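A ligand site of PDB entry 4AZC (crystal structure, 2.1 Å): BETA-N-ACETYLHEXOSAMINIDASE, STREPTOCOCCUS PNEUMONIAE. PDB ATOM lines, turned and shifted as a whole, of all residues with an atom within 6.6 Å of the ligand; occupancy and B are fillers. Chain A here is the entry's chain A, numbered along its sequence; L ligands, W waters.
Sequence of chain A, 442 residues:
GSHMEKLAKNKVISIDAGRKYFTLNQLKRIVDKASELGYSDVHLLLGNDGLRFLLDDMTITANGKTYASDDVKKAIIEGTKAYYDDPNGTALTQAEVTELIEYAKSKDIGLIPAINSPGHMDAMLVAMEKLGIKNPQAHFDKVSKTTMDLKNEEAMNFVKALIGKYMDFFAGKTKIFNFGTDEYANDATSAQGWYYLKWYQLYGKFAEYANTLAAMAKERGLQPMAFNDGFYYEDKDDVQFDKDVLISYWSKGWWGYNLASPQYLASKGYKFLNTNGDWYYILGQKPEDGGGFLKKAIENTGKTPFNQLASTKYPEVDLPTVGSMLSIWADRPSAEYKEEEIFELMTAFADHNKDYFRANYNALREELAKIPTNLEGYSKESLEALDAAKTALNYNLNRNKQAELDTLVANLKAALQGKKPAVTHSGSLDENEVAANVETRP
O1 of the ligand sits at hydrogen-bond distance from OD1 of Asp 331, 2.6 Å away. An oxygen (O1) of the ligand is in hydrogen-bond range of the guanidinium group (NH1) of Arg 19, at 2.7 Å. A nitrogen (N1) of the ligand lies within salt-bridge range of the side-chain carboxylate of Glu 183 (3.5 Å). A nitrogen (N1) of the ligand lies within salt-bridge range of the side-chain carboxylate (OD2) of Asp 182 (2.7 Å). The side-chain hydroxyl (OH) of Tyr 280 lies close to a sulfur (S1) of the ligand.
The side-chain amide nitrogen (ND2) of Asn 116 lies within hydrogen-bond range of the side-chain carboxylate (OD1) of Asp 182. The backbone carbonyl oxygen (O) of Tyr 281 is in hydrogen-bond range of the backbone NH (N) of Trp 329 (2.9 Å). The backbone carbonyl oxygen (O) of Asn 48 sits at hydrogen-bond distance from the backbone NH (N) of Arg 19. The backbone carbonyl oxygen (O) of His 120 is in hydrogen-bond range of the backbone NH (N) of Asp 49, at 2.8 Å. OE1 of Glu 183 is in hydrogen-bond range of NE2 of His 120 (2.9 Å). The side-chain carboxylate of Asp 182 is in hydrogen-bond range of a ring nitrogen (NE2) of His 120 (3.1 Å). The side-chain carboxylate (OD2) of Asp 16 is in salt-bridge range of the guanidinium group (NH1) of Arg 19. The side-chain amide nitrogen of Asn 186 is in hydrogen-bond range of the side-chain carboxylate of Glu 183 (3.3 Å).
Residues that only touch the ligand: His 120 (3.4 Å), Phe 227 (3.6 Å), Trp 250 (3.5 Å), Ile 282 (3.5 Å) and Trp 329 (3.3 Å). Within 4 Å of the ligand: Arg 19, His 120, Asp 182, Glu 183, Phe 227, Trp 250, Tyr 280, Ile 282, Trp 329 and Asp 331.
Water W1 lies within hydrogen-bond range of O2 of the ligand (2.7 Å), OD2 of Asp 182 (2.8 Å) and ND2 of Asn 48 (2.9 Å).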
ATOM      1  N   ASP A  16      12.114  -6.182  15.442  1.00  0.00           N
ATOM      2  CA  ASP A  16      12.732  -7.307  14.741  1.00  0.00           C
ATOM      3  C   ASP A  16      13.457  -8.195  15.757  1.00  0.00           C
ATOM      4  O   ASP A  16      14.682  -8.082  15.955  1.00  0.00           O
ATOM      5  CB  ASP A  16      13.670  -6.792  13.638  1.00  0.00           C
ATOM      6  CG  ASP A  16      14.307  -7.907  12.803  1.00  0.00           C
ATOM      7  OD1 ASP A  16      13.986  -9.100  12.997  1.00  0.00           O
ATOM      8  OD2 ASP A  16      15.172  -7.598  11.943  1.00  0.00           O
ATOM      9  N   ARG A  19      15.870 -11.480  13.762  1.00  0.00           N
ATOM     10  CA  ARG A  19      17.300 -11.449  13.454  1.00  0.00           C
ATOM     11  C   ARG A  19      18.144 -11.408  14.729  1.00  0.00           C
ATOM     12  O   ARG A  19      19.225 -12.017  14.790  1.00  0.00           O
ATOM     13  CB  ARG A  19      17.649 -10.265  12.564  1.00  0.00           C
ATOM     14  CG  ARG A  19      17.034 -10.335  11.166  1.00  0.00           C
ATOM     15  CD  ARG A  19      17.637  -9.209  10.350  1.00  0.00           C
ATOM     16  NE  ARG A  19      17.340  -9.253   8.929  1.00  0.00           N
ATOM     17  CZ  ARG A  19      16.402  -8.525   8.332  1.00  0.00           C
ATOM     18  NH1 ARG A  19      15.610  -7.715   9.045  1.00  0.00           N
ATOM     19  NH2 ARG A  19      16.258  -8.594   7.017  1.00  0.00           N
ATOM     20  N   ASN A  48      12.250 -14.243  11.462  1.00  0.00           N
ATOM     21  CA  ASN A  48      12.727 -13.243  10.505  1.00  0.00           C
ATOM     22  C   ASN A  48      14.211 -13.467  10.391  1.00  0.00           C
ATOM     23  O   ASN A  48      14.983 -12.944  11.217  1.00  0.00           O
ATOM     24  CB  ASN A  48      12.437 -11.825  10.985  1.00  0.00           C
ATOM     25  CG  ASN A  48      12.562 -10.796   9.882  1.00  0.00           C
ATOM     26  OD1 ASN A  48      13.162  -9.746  10.079  1.00  0.00           O
ATOM     27  ND2 ASN A  48      11.977 -11.084   8.728  1.00  0.00           N
ATOM     28  N   ASP A  49      14.597 -14.268   9.397  1.00  0.00           N
ATOM     29  CA  ASP A  49      15.945 -14.834   9.234  1.00  0.00           C
ATOM     30  C   ASP A  49      16.212 -15.847  10.348  1.00  0.00           C
ATOM     31  O   ASP A  49      16.173 -17.059  10.113  1.00  0.00           O
ATOM     32  CB  ASP A  49      17.042 -13.762   9.188  1.00  0.00           C
ATOM     33  CG  ASP A  49      16.915 -12.843   7.989  1.00  0.00           C
ATOM     34  OD1 ASP A  49      15.888 -12.905   7.295  1.00  0.00           O
ATOM     35  OD2 ASP A  49      17.848 -12.055   7.731  1.00  0.00           O
ATOM     36  N   ASN A 116       8.091 -15.304   9.541  1.00  0.00           N
ATOM     37  CA  ASN A 116       8.263 -15.044   8.097  1.00  0.00           C
ATOM     38  C   ASN A 116       8.526 -16.310   7.299  1.00  0.00           C
ATOM     39  O   ASN A 116       9.265 -17.179   7.751  1.00  0.00           O
ATOM     40  CB  ASN A 116       9.416 -14.039   7.867  1.00  0.00           C
ATOM     41  CG  ASN A 116       9.117 -13.050   6.734  1.00  0.00           C
ATOM     42  OD1 ASN A 116       8.397 -13.353   5.782  1.00  0.00           O
ATOM     43  ND2 ASN A 116       9.690 -11.850   6.835  1.00  0.00           N
ATOM     44  N   HIS A 120      13.155 -14.734   4.107  1.00  0.00           N
ATOM     45  CA  HIS A 120      13.580 -14.417   5.472  1.00  0.00           C
ATOM     46  C   HIS A 120      13.409 -15.622   6.449  1.00  0.00           C
ATOM     47  O   HIS A 120      12.876 -15.472   7.562  1.00  0.00           O
ATOM     48  CB  HIS A 120      12.851 -13.160   5.978  1.00  0.00           C
ATOM     49  CG  HIS A 120      13.250 -11.899   5.274  1.00  0.00           C
ATOM     50  ND1 HIS A 120      14.470 -11.284   5.473  1.00  0.00           N
ATOM     51  CD2 HIS A 120      12.580 -11.129   4.389  1.00  0.00           C
ATOM     52  CE1 HIS A 120      14.539 -10.194   4.725  1.00  0.00           C
ATOM     53  NE2 HIS A 120      13.402 -10.069   4.068  1.00  0.00           N
ATOM     54  N   ASP A 182       7.544 -10.994   2.443  1.00  0.00           N
ATOM     55  CA  ASP A 182       8.369  -9.954   1.825  1.00  0.00           C
ATOM     56  C   ASP A 182       9.645 -10.488   1.163  1.00  0.00           C
ATOM     57  O   ASP A 182      10.154 -11.558   1.525  1.00  0.00           O
ATOM     58  CB  ASP A 182       8.725  -8.862   2.857  1.00  0.00           C
ATOM     59  CG  ASP A 182       9.603  -9.375   3.978  1.00  0.00           C
ATOM     60  OD1 ASP A 182       9.250 -10.409   4.572  1.00  0.00           O
ATOM     61  OD2 ASP A 182      10.634  -8.733   4.307  1.00  0.00           O
ATOM     62  N   GLU A 183      10.133  -9.719   0.181  1.00  0.00           N
ATOM     63  CA  GLU A 183      11.479  -9.885  -0.400  1.00  0.00           C
ATOM     64  C   GLU A 183      11.905 -11.327  -0.773  1.00  0.00           C
ATOM     65  O   GLU A 183      13.027 -11.756  -0.414  1.00  0.00           O
ATOM     66  CB  GLU A 183      12.525  -9.217   0.522  1.00  0.00           C
ATOM     67  CG  GLU A 183      12.458  -7.653   0.565  1.00  0.00           C
ATOM     68  CD  GLU A 183      13.471  -7.013   1.546  1.00  0.00           C
ATOM     69  OE1 GLU A 183      13.882  -7.675   2.531  1.00  0.00           O
ATOM     70  OE2 GLU A 183      13.847  -5.852   1.306  1.00  0.00           O
ATOM     71  N   ASN A 186      15.693 -12.427  -2.248  1.00  0.00           N
ATOM     72  CA  ASN A 186      16.480 -11.228  -2.552  1.00  0.00           C
ATOM     73  C   ASN A 186      17.978 -11.533  -2.694  1.00  0.00           C
ATOM     74  O   ASN A 186      18.616 -11.047  -3.629  1.00  0.00           O
ATOM     75  CB  ASN A 186      16.180 -10.028  -1.615  1.00  0.00           C
ATOM     76  CG  ASN A 186      16.423 -10.326  -0.112  1.00  0.00           C
ATOM     77  OD1 ASN A 186      16.836 -11.416   0.267  1.00  0.00           O
ATOM     78  ND2 ASN A 186      16.131  -9.336   0.731  1.00  0.00           N
ATOM     79  N   PHE A 227       3.169  -8.574   4.437  1.00  0.00           N
ATOM     80  CA  PHE A 227       3.744  -7.397   3.773  1.00  0.00           C
ATOM     81  C   PHE A 227       3.271  -7.359   2.326  1.00  0.00           C
ATOM     82  O   PHE A 227       2.855  -8.379   1.779  1.00  0.00           O
ATOM     83  CB  PHE A 227       5.273  -7.413   3.868  1.00  0.00           C
ATOM     84  CG  PHE A 227       5.770  -7.353   5.283  1.00  0.00           C
ATOM     85  CD1 PHE A 227       5.494  -6.243   6.081  1.00  0.00           C
ATOM     86  CD2 PHE A 227       6.515  -8.404   5.818  1.00  0.00           C
ATOM     87  CE1 PHE A 227       5.928  -6.178   7.402  1.00  0.00           C
ATOM     88  CE2 PHE A 227       6.972  -8.340   7.146  1.00  0.00           C
ATOM     89  CZ  PHE A 227       6.660  -7.237   7.936  1.00  0.00           C
ATOM     90  N   ASP A 229       4.773  -6.797  -0.645  1.00  0.00           N
ATOM     91  CA  ASP A 229       5.663  -7.157  -1.751  1.00  0.00           C
ATOM     92  C   ASP A 229       5.075  -8.108  -2.792  1.00  0.00           C
ATOM     93  O   ASP A 229       5.051  -7.789  -3.979  1.00  0.00           O
ATOM     94  CB  ASP A 229       6.957  -7.783  -1.229  1.00  0.00           C
ATOM     95  CG  ASP A 229       7.679  -6.874  -0.257  1.00  0.00           C
ATOM     96  OD1 ASP A 229       6.983  -6.265   0.603  1.00  0.00           O
ATOM     97  OD2 ASP A 229       8.919  -6.786  -0.351  1.00  0.00           O
ATOM     98  N   SER A 248       0.398  -5.031   5.357  1.00  0.00           N
ATOM     99  CA  SER A 248       1.421  -4.135   5.924  1.00  0.00           C
ATOM    100  C   SER A 248       2.182  -3.509   4.750  1.00  0.00           C
ATOM    101  O   SER A 248       3.083  -4.145   4.178  1.00  0.00           O
ATOM    102  CB  SER A 248       2.347  -4.910   6.842  1.00  0.00           C
ATOM    103  OG  SER A 248       3.337  -4.087   7.403  1.00  0.00           O
ATOM    104  N   TRP A 250       4.658  -0.979   2.936  1.00  0.00           N
ATOM    105  CA  TRP A 250       5.872  -0.268   3.374  1.00  0.00           C
ATOM    106  C   TRP A 250       6.656   0.448   2.289  1.00  0.00           C
ATOM    107  O   TRP A 250       7.415   1.374   2.575  1.00  0.00           O
ATOM    108  CB  TRP A 250       6.783  -1.204   4.178  1.00  0.00           C
ATOM    109  CG  TRP A 250       7.470  -2.248   3.349  1.00  0.00           C
ATOM    110  CD1 TRP A 250       6.944  -3.443   2.949  1.00  0.00           C
ATOM    111  CD2 TRP A 250       8.798  -2.192   2.828  1.00  0.00           C
ATOM    112  NE1 TRP A 250       7.879  -4.137   2.208  1.00  0.00           N
ATOM    113  CE2 TRP A 250       9.017  -3.390   2.098  1.00  0.00           C
ATOM    114  CE3 TRP A 250       9.834  -1.240   2.888  1.00  0.00           C
ATOM    115  CZ2 TRP A 250      10.234  -3.658   1.439  1.00  0.00           C
ATOM    116  CZ3 TRP A 250      11.038  -1.512   2.213  1.00  0.00           C
ATOM    117  CH2 TRP A 250      11.216  -2.713   1.504  1.00  0.00           C
ATOM    118  N   TRP A 254      11.581  -0.275  -5.952  1.00  0.00           N
ATOM    119  CA  TRP A 254      12.647   0.553  -6.509  1.00  0.00           C
ATOM    120  C   TRP A 254      12.924   0.038  -7.922  1.00  0.00           C
ATOM    121  O   TRP A 254      12.225  -0.872  -8.391  1.00  0.00           O
ATOM    122  CB  TRP A 254      13.901   0.479  -5.633  1.00  0.00           C
ATOM    123  CG  TRP A 254      14.236  -0.915  -5.202  1.00  0.00           C
ATOM    124  CD1 TRP A 254      14.991  -1.828  -5.899  1.00  0.00           C
ATOM    125  CD2 TRP A 254      13.838  -1.570  -3.983  1.00  0.00           C
ATOM    126  NE1 TRP A 254      15.079  -3.011  -5.185  1.00  0.00           N
ATOM    127  CE2 TRP A 254      14.387  -2.878  -4.006  1.00  0.00           C
ATOM    128  CE3 TRP A 254      13.093  -1.169  -2.859  1.00  0.00           C
ATOM    129  CZ2 TRP A 254      14.199  -3.805  -2.959  1.00  0.00           C
ATOM    130  CZ3 TRP A 254      12.888  -2.094  -1.812  1.00  0.00           C
ATOM    131  CH2 TRP A 254      13.450  -3.388  -1.876  1.00  0.00           C
ATOM    132  N   TYR A 280      11.376   3.872   9.382  1.00  0.00           N
ATOM    133  CA  TYR A 280      12.303   2.792   9.780  1.00  0.00           C
ATOM    134  C   TYR A 280      13.558   3.265  10.472  1.00  0.00           C
ATOM    135  O   TYR A 280      14.184   4.254  10.077  1.00  0.00           O
ATOM    136  CB  TYR A 280      12.790   2.003   8.561  1.00  0.00           C
ATOM    137  CG  TYR A 280      11.771   1.099   7.914  1.00  0.00           C
ATOM    138  CD1 TYR A 280      10.503   0.919   8.472  1.00  0.00           C
ATOM    139  CD2 TYR A 280      12.096   0.409   6.744  1.00  0.00           C
ATOM    140  CE1 TYR A 280       9.569   0.078   7.859  1.00  0.00           C
ATOM    141  CE2 TYR A 280      11.186  -0.422   6.148  1.00  0.00           C
ATOM    142  CZ  TYR A 280       9.926  -0.584   6.696  1.00  0.00           C
ATOM    143  OH  TYR A 280       9.032  -1.427   6.090  1.00  0.00           O
ATOM    144  N   TYR A 281      13.928   2.514  11.512  1.00  0.00           N
ATOM    145  CA  TYR A 281      15.257   2.575  12.097  1.00  0.00           C
ATOM    146  C   TYR A 281      15.858   1.175  12.109  1.00  0.00           C
ATOM    147  O   TYR A 281      15.243   0.232  12.613  1.00  0.00           O
ATOM    148  CB  TYR A 281      15.229   3.166  13.514  1.00  0.00           C
ATOM    149  CG  TYR A 281      16.575   3.126  14.204  1.00  0.00           C
ATOM    150  CD1 TYR A 281      17.710   3.680  13.586  1.00  0.00           C
ATOM    151  CD2 TYR A 281      16.729   2.554  15.472  1.00  0.00           C
ATOM    152  CE1 TYR A 281      18.965   3.658  14.213  1.00  0.00           C
ATOM    153  CE2 TYR A 281      17.993   2.513  16.110  1.00  0.00           C
ATOM    154  CZ  TYR A 281      19.089   3.072  15.470  1.00  0.00           C
ATOM    155  OH  TYR A 281      20.327   3.055  16.083  1.00  0.00           O
ATOM    156  N   ILE A 282      17.042   1.063  11.512  1.00  0.00           N
ATOM    157  CA  ILE A 282      17.835  -0.160  11.495  1.00  0.00           C
ATOM    158  C   ILE A 282      18.884   0.033  12.592  1.00  0.00           C
ATOM    159  O   ILE A 282      19.608   1.045  12.585  1.00  0.00           O
ATOM    160  CB  ILE A 282      18.506  -0.364  10.116  1.00  0.00           C
ATOM    161  CG1 ILE A 282      17.440  -0.552   9.005  1.00  0.00           C
ATOM    162  CG2 ILE A 282      19.480  -1.531  10.149  1.00  0.00           C
ATOM    163  CD1 ILE A 282      17.988  -0.400   7.564  1.00  0.00           C
ATOM    164  N   TRP A 329      14.277  -2.457  12.867  1.00  0.00           N
ATOM    165  CA  TRP A 329      14.838  -3.617  12.195  1.00  0.00           C
ATOM    166  C   TRP A 329      16.247  -3.889  12.688  1.00  0.00           C
ATOM    167  O   TRP A 329      16.966  -2.959  13.096  1.00  0.00           O
ATOM    168  CB  TRP A 329      14.857  -3.416  10.680  1.00  0.00           C
ATOM    169  CG  TRP A 329      13.501  -3.179  10.089  1.00  0.00           C
ATOM    170  CD1 TRP A 329      12.963  -1.974   9.714  1.00  0.00           C
ATOM    171  CD2 TRP A 329      12.495  -4.173   9.821  1.00  0.00           C
ATOM    172  NE1 TRP A 329      11.687  -2.158   9.223  1.00  0.00           N
ATOM    173  CE2 TRP A 329      11.370  -3.499   9.282  1.00  0.00           C
ATOM    174  CE3 TRP A 329      12.433  -5.566   9.992  1.00  0.00           C
ATOM    175  CZ2 TRP A 329      10.214  -4.165   8.904  1.00  0.00           C
ATOM    176  CZ3 TRP A 329      11.265  -6.239   9.611  1.00  0.00           C
ATOM    177  CH2 TRP A 329      10.168  -5.528   9.080  1.00  0.00           C
ATOM    178  N   ALA A 330      16.656  -5.147  12.606  1.00  0.00           N
ATOM    179  CA  ALA A 330      17.999  -5.530  13.063  1.00  0.00           C
ATOM    180  C   ALA A 330      18.854  -6.211  11.979  1.00  0.00           C
ATOM    181  O   ALA A 330      19.486  -7.234  12.244  1.00  0.00           O
ATOM    182  CB  ALA A 330      17.909  -6.374  14.350  1.00  0.00           C
ATOM    183  N   ASP A 331      18.871  -5.615  10.777  1.00  0.00           N
ATOM    184  CA  ASP A 331      19.624  -6.142   9.602  1.00  0.00           C
ATOM    185  C   ASP A 331      21.036  -6.616   9.938  1.00  0.00           C
ATOM    186  O   ASP A 331      21.491  -7.653   9.421  1.00  0.00           O
ATOM    187  CB  ASP A 331      19.704  -5.097   8.466  1.00  0.00           C
ATOM    188  CG  ASP A 331      18.330  -4.736   7.896  1.00  0.00           C
ATOM    189  OD1 ASP A 331      17.334  -4.745   8.663  1.00  0.00           O
ATOM    190  OD2 ASP A 331      18.241  -4.426   6.685  1.00  0.00           O
HETATM  191  O1  LIG L   1      14.964  -5.339   7.832  1.00  0.00           O
HETATM  192  C1  LIG L   1      14.527  -5.015   6.515  1.00  0.00           C
HETATM  193  C2  LIG L   1      13.338  -5.892   6.192  1.00  0.00           C
HETATM  194  C3  LIG L   1      14.127  -3.553   6.432  1.00  0.00           C
HETATM  195  O2  LIG L   1      13.720  -7.281   6.323  1.00  0.00           O
HETATM  196  C4  LIG L   1      12.779  -5.573   4.778  1.00  0.00           C
HETATM  197  N1  LIG L   1      11.458  -6.202   4.545  1.00  0.00           N
HETATM  198  C5  LIG L   1      12.549  -4.045   4.581  1.00  0.00           C
HETATM  199  C6  LIG L   1      10.480  -5.573   5.467  1.00  0.00           C
HETATM  200  C7  LIG L   1       9.046  -5.862   5.026  1.00  0.00           C
HETATM  201  S1  LIG L   1      10.915  -3.808   5.384  1.00  0.00           S
HETATM  202  O3  LIG L   1      13.632  -3.181   5.122  1.00  0.00           O
HETATM  203  C8  LIG L   1      15.312  -2.612   6.702  1.00  0.00           C
HETATM  204  O4  LIG L   1      16.357  -2.857   5.755  1.00  0.00           O
HETATM  205  O   HOH W   1      11.678  -8.861   6.928  1.00  0.00           O
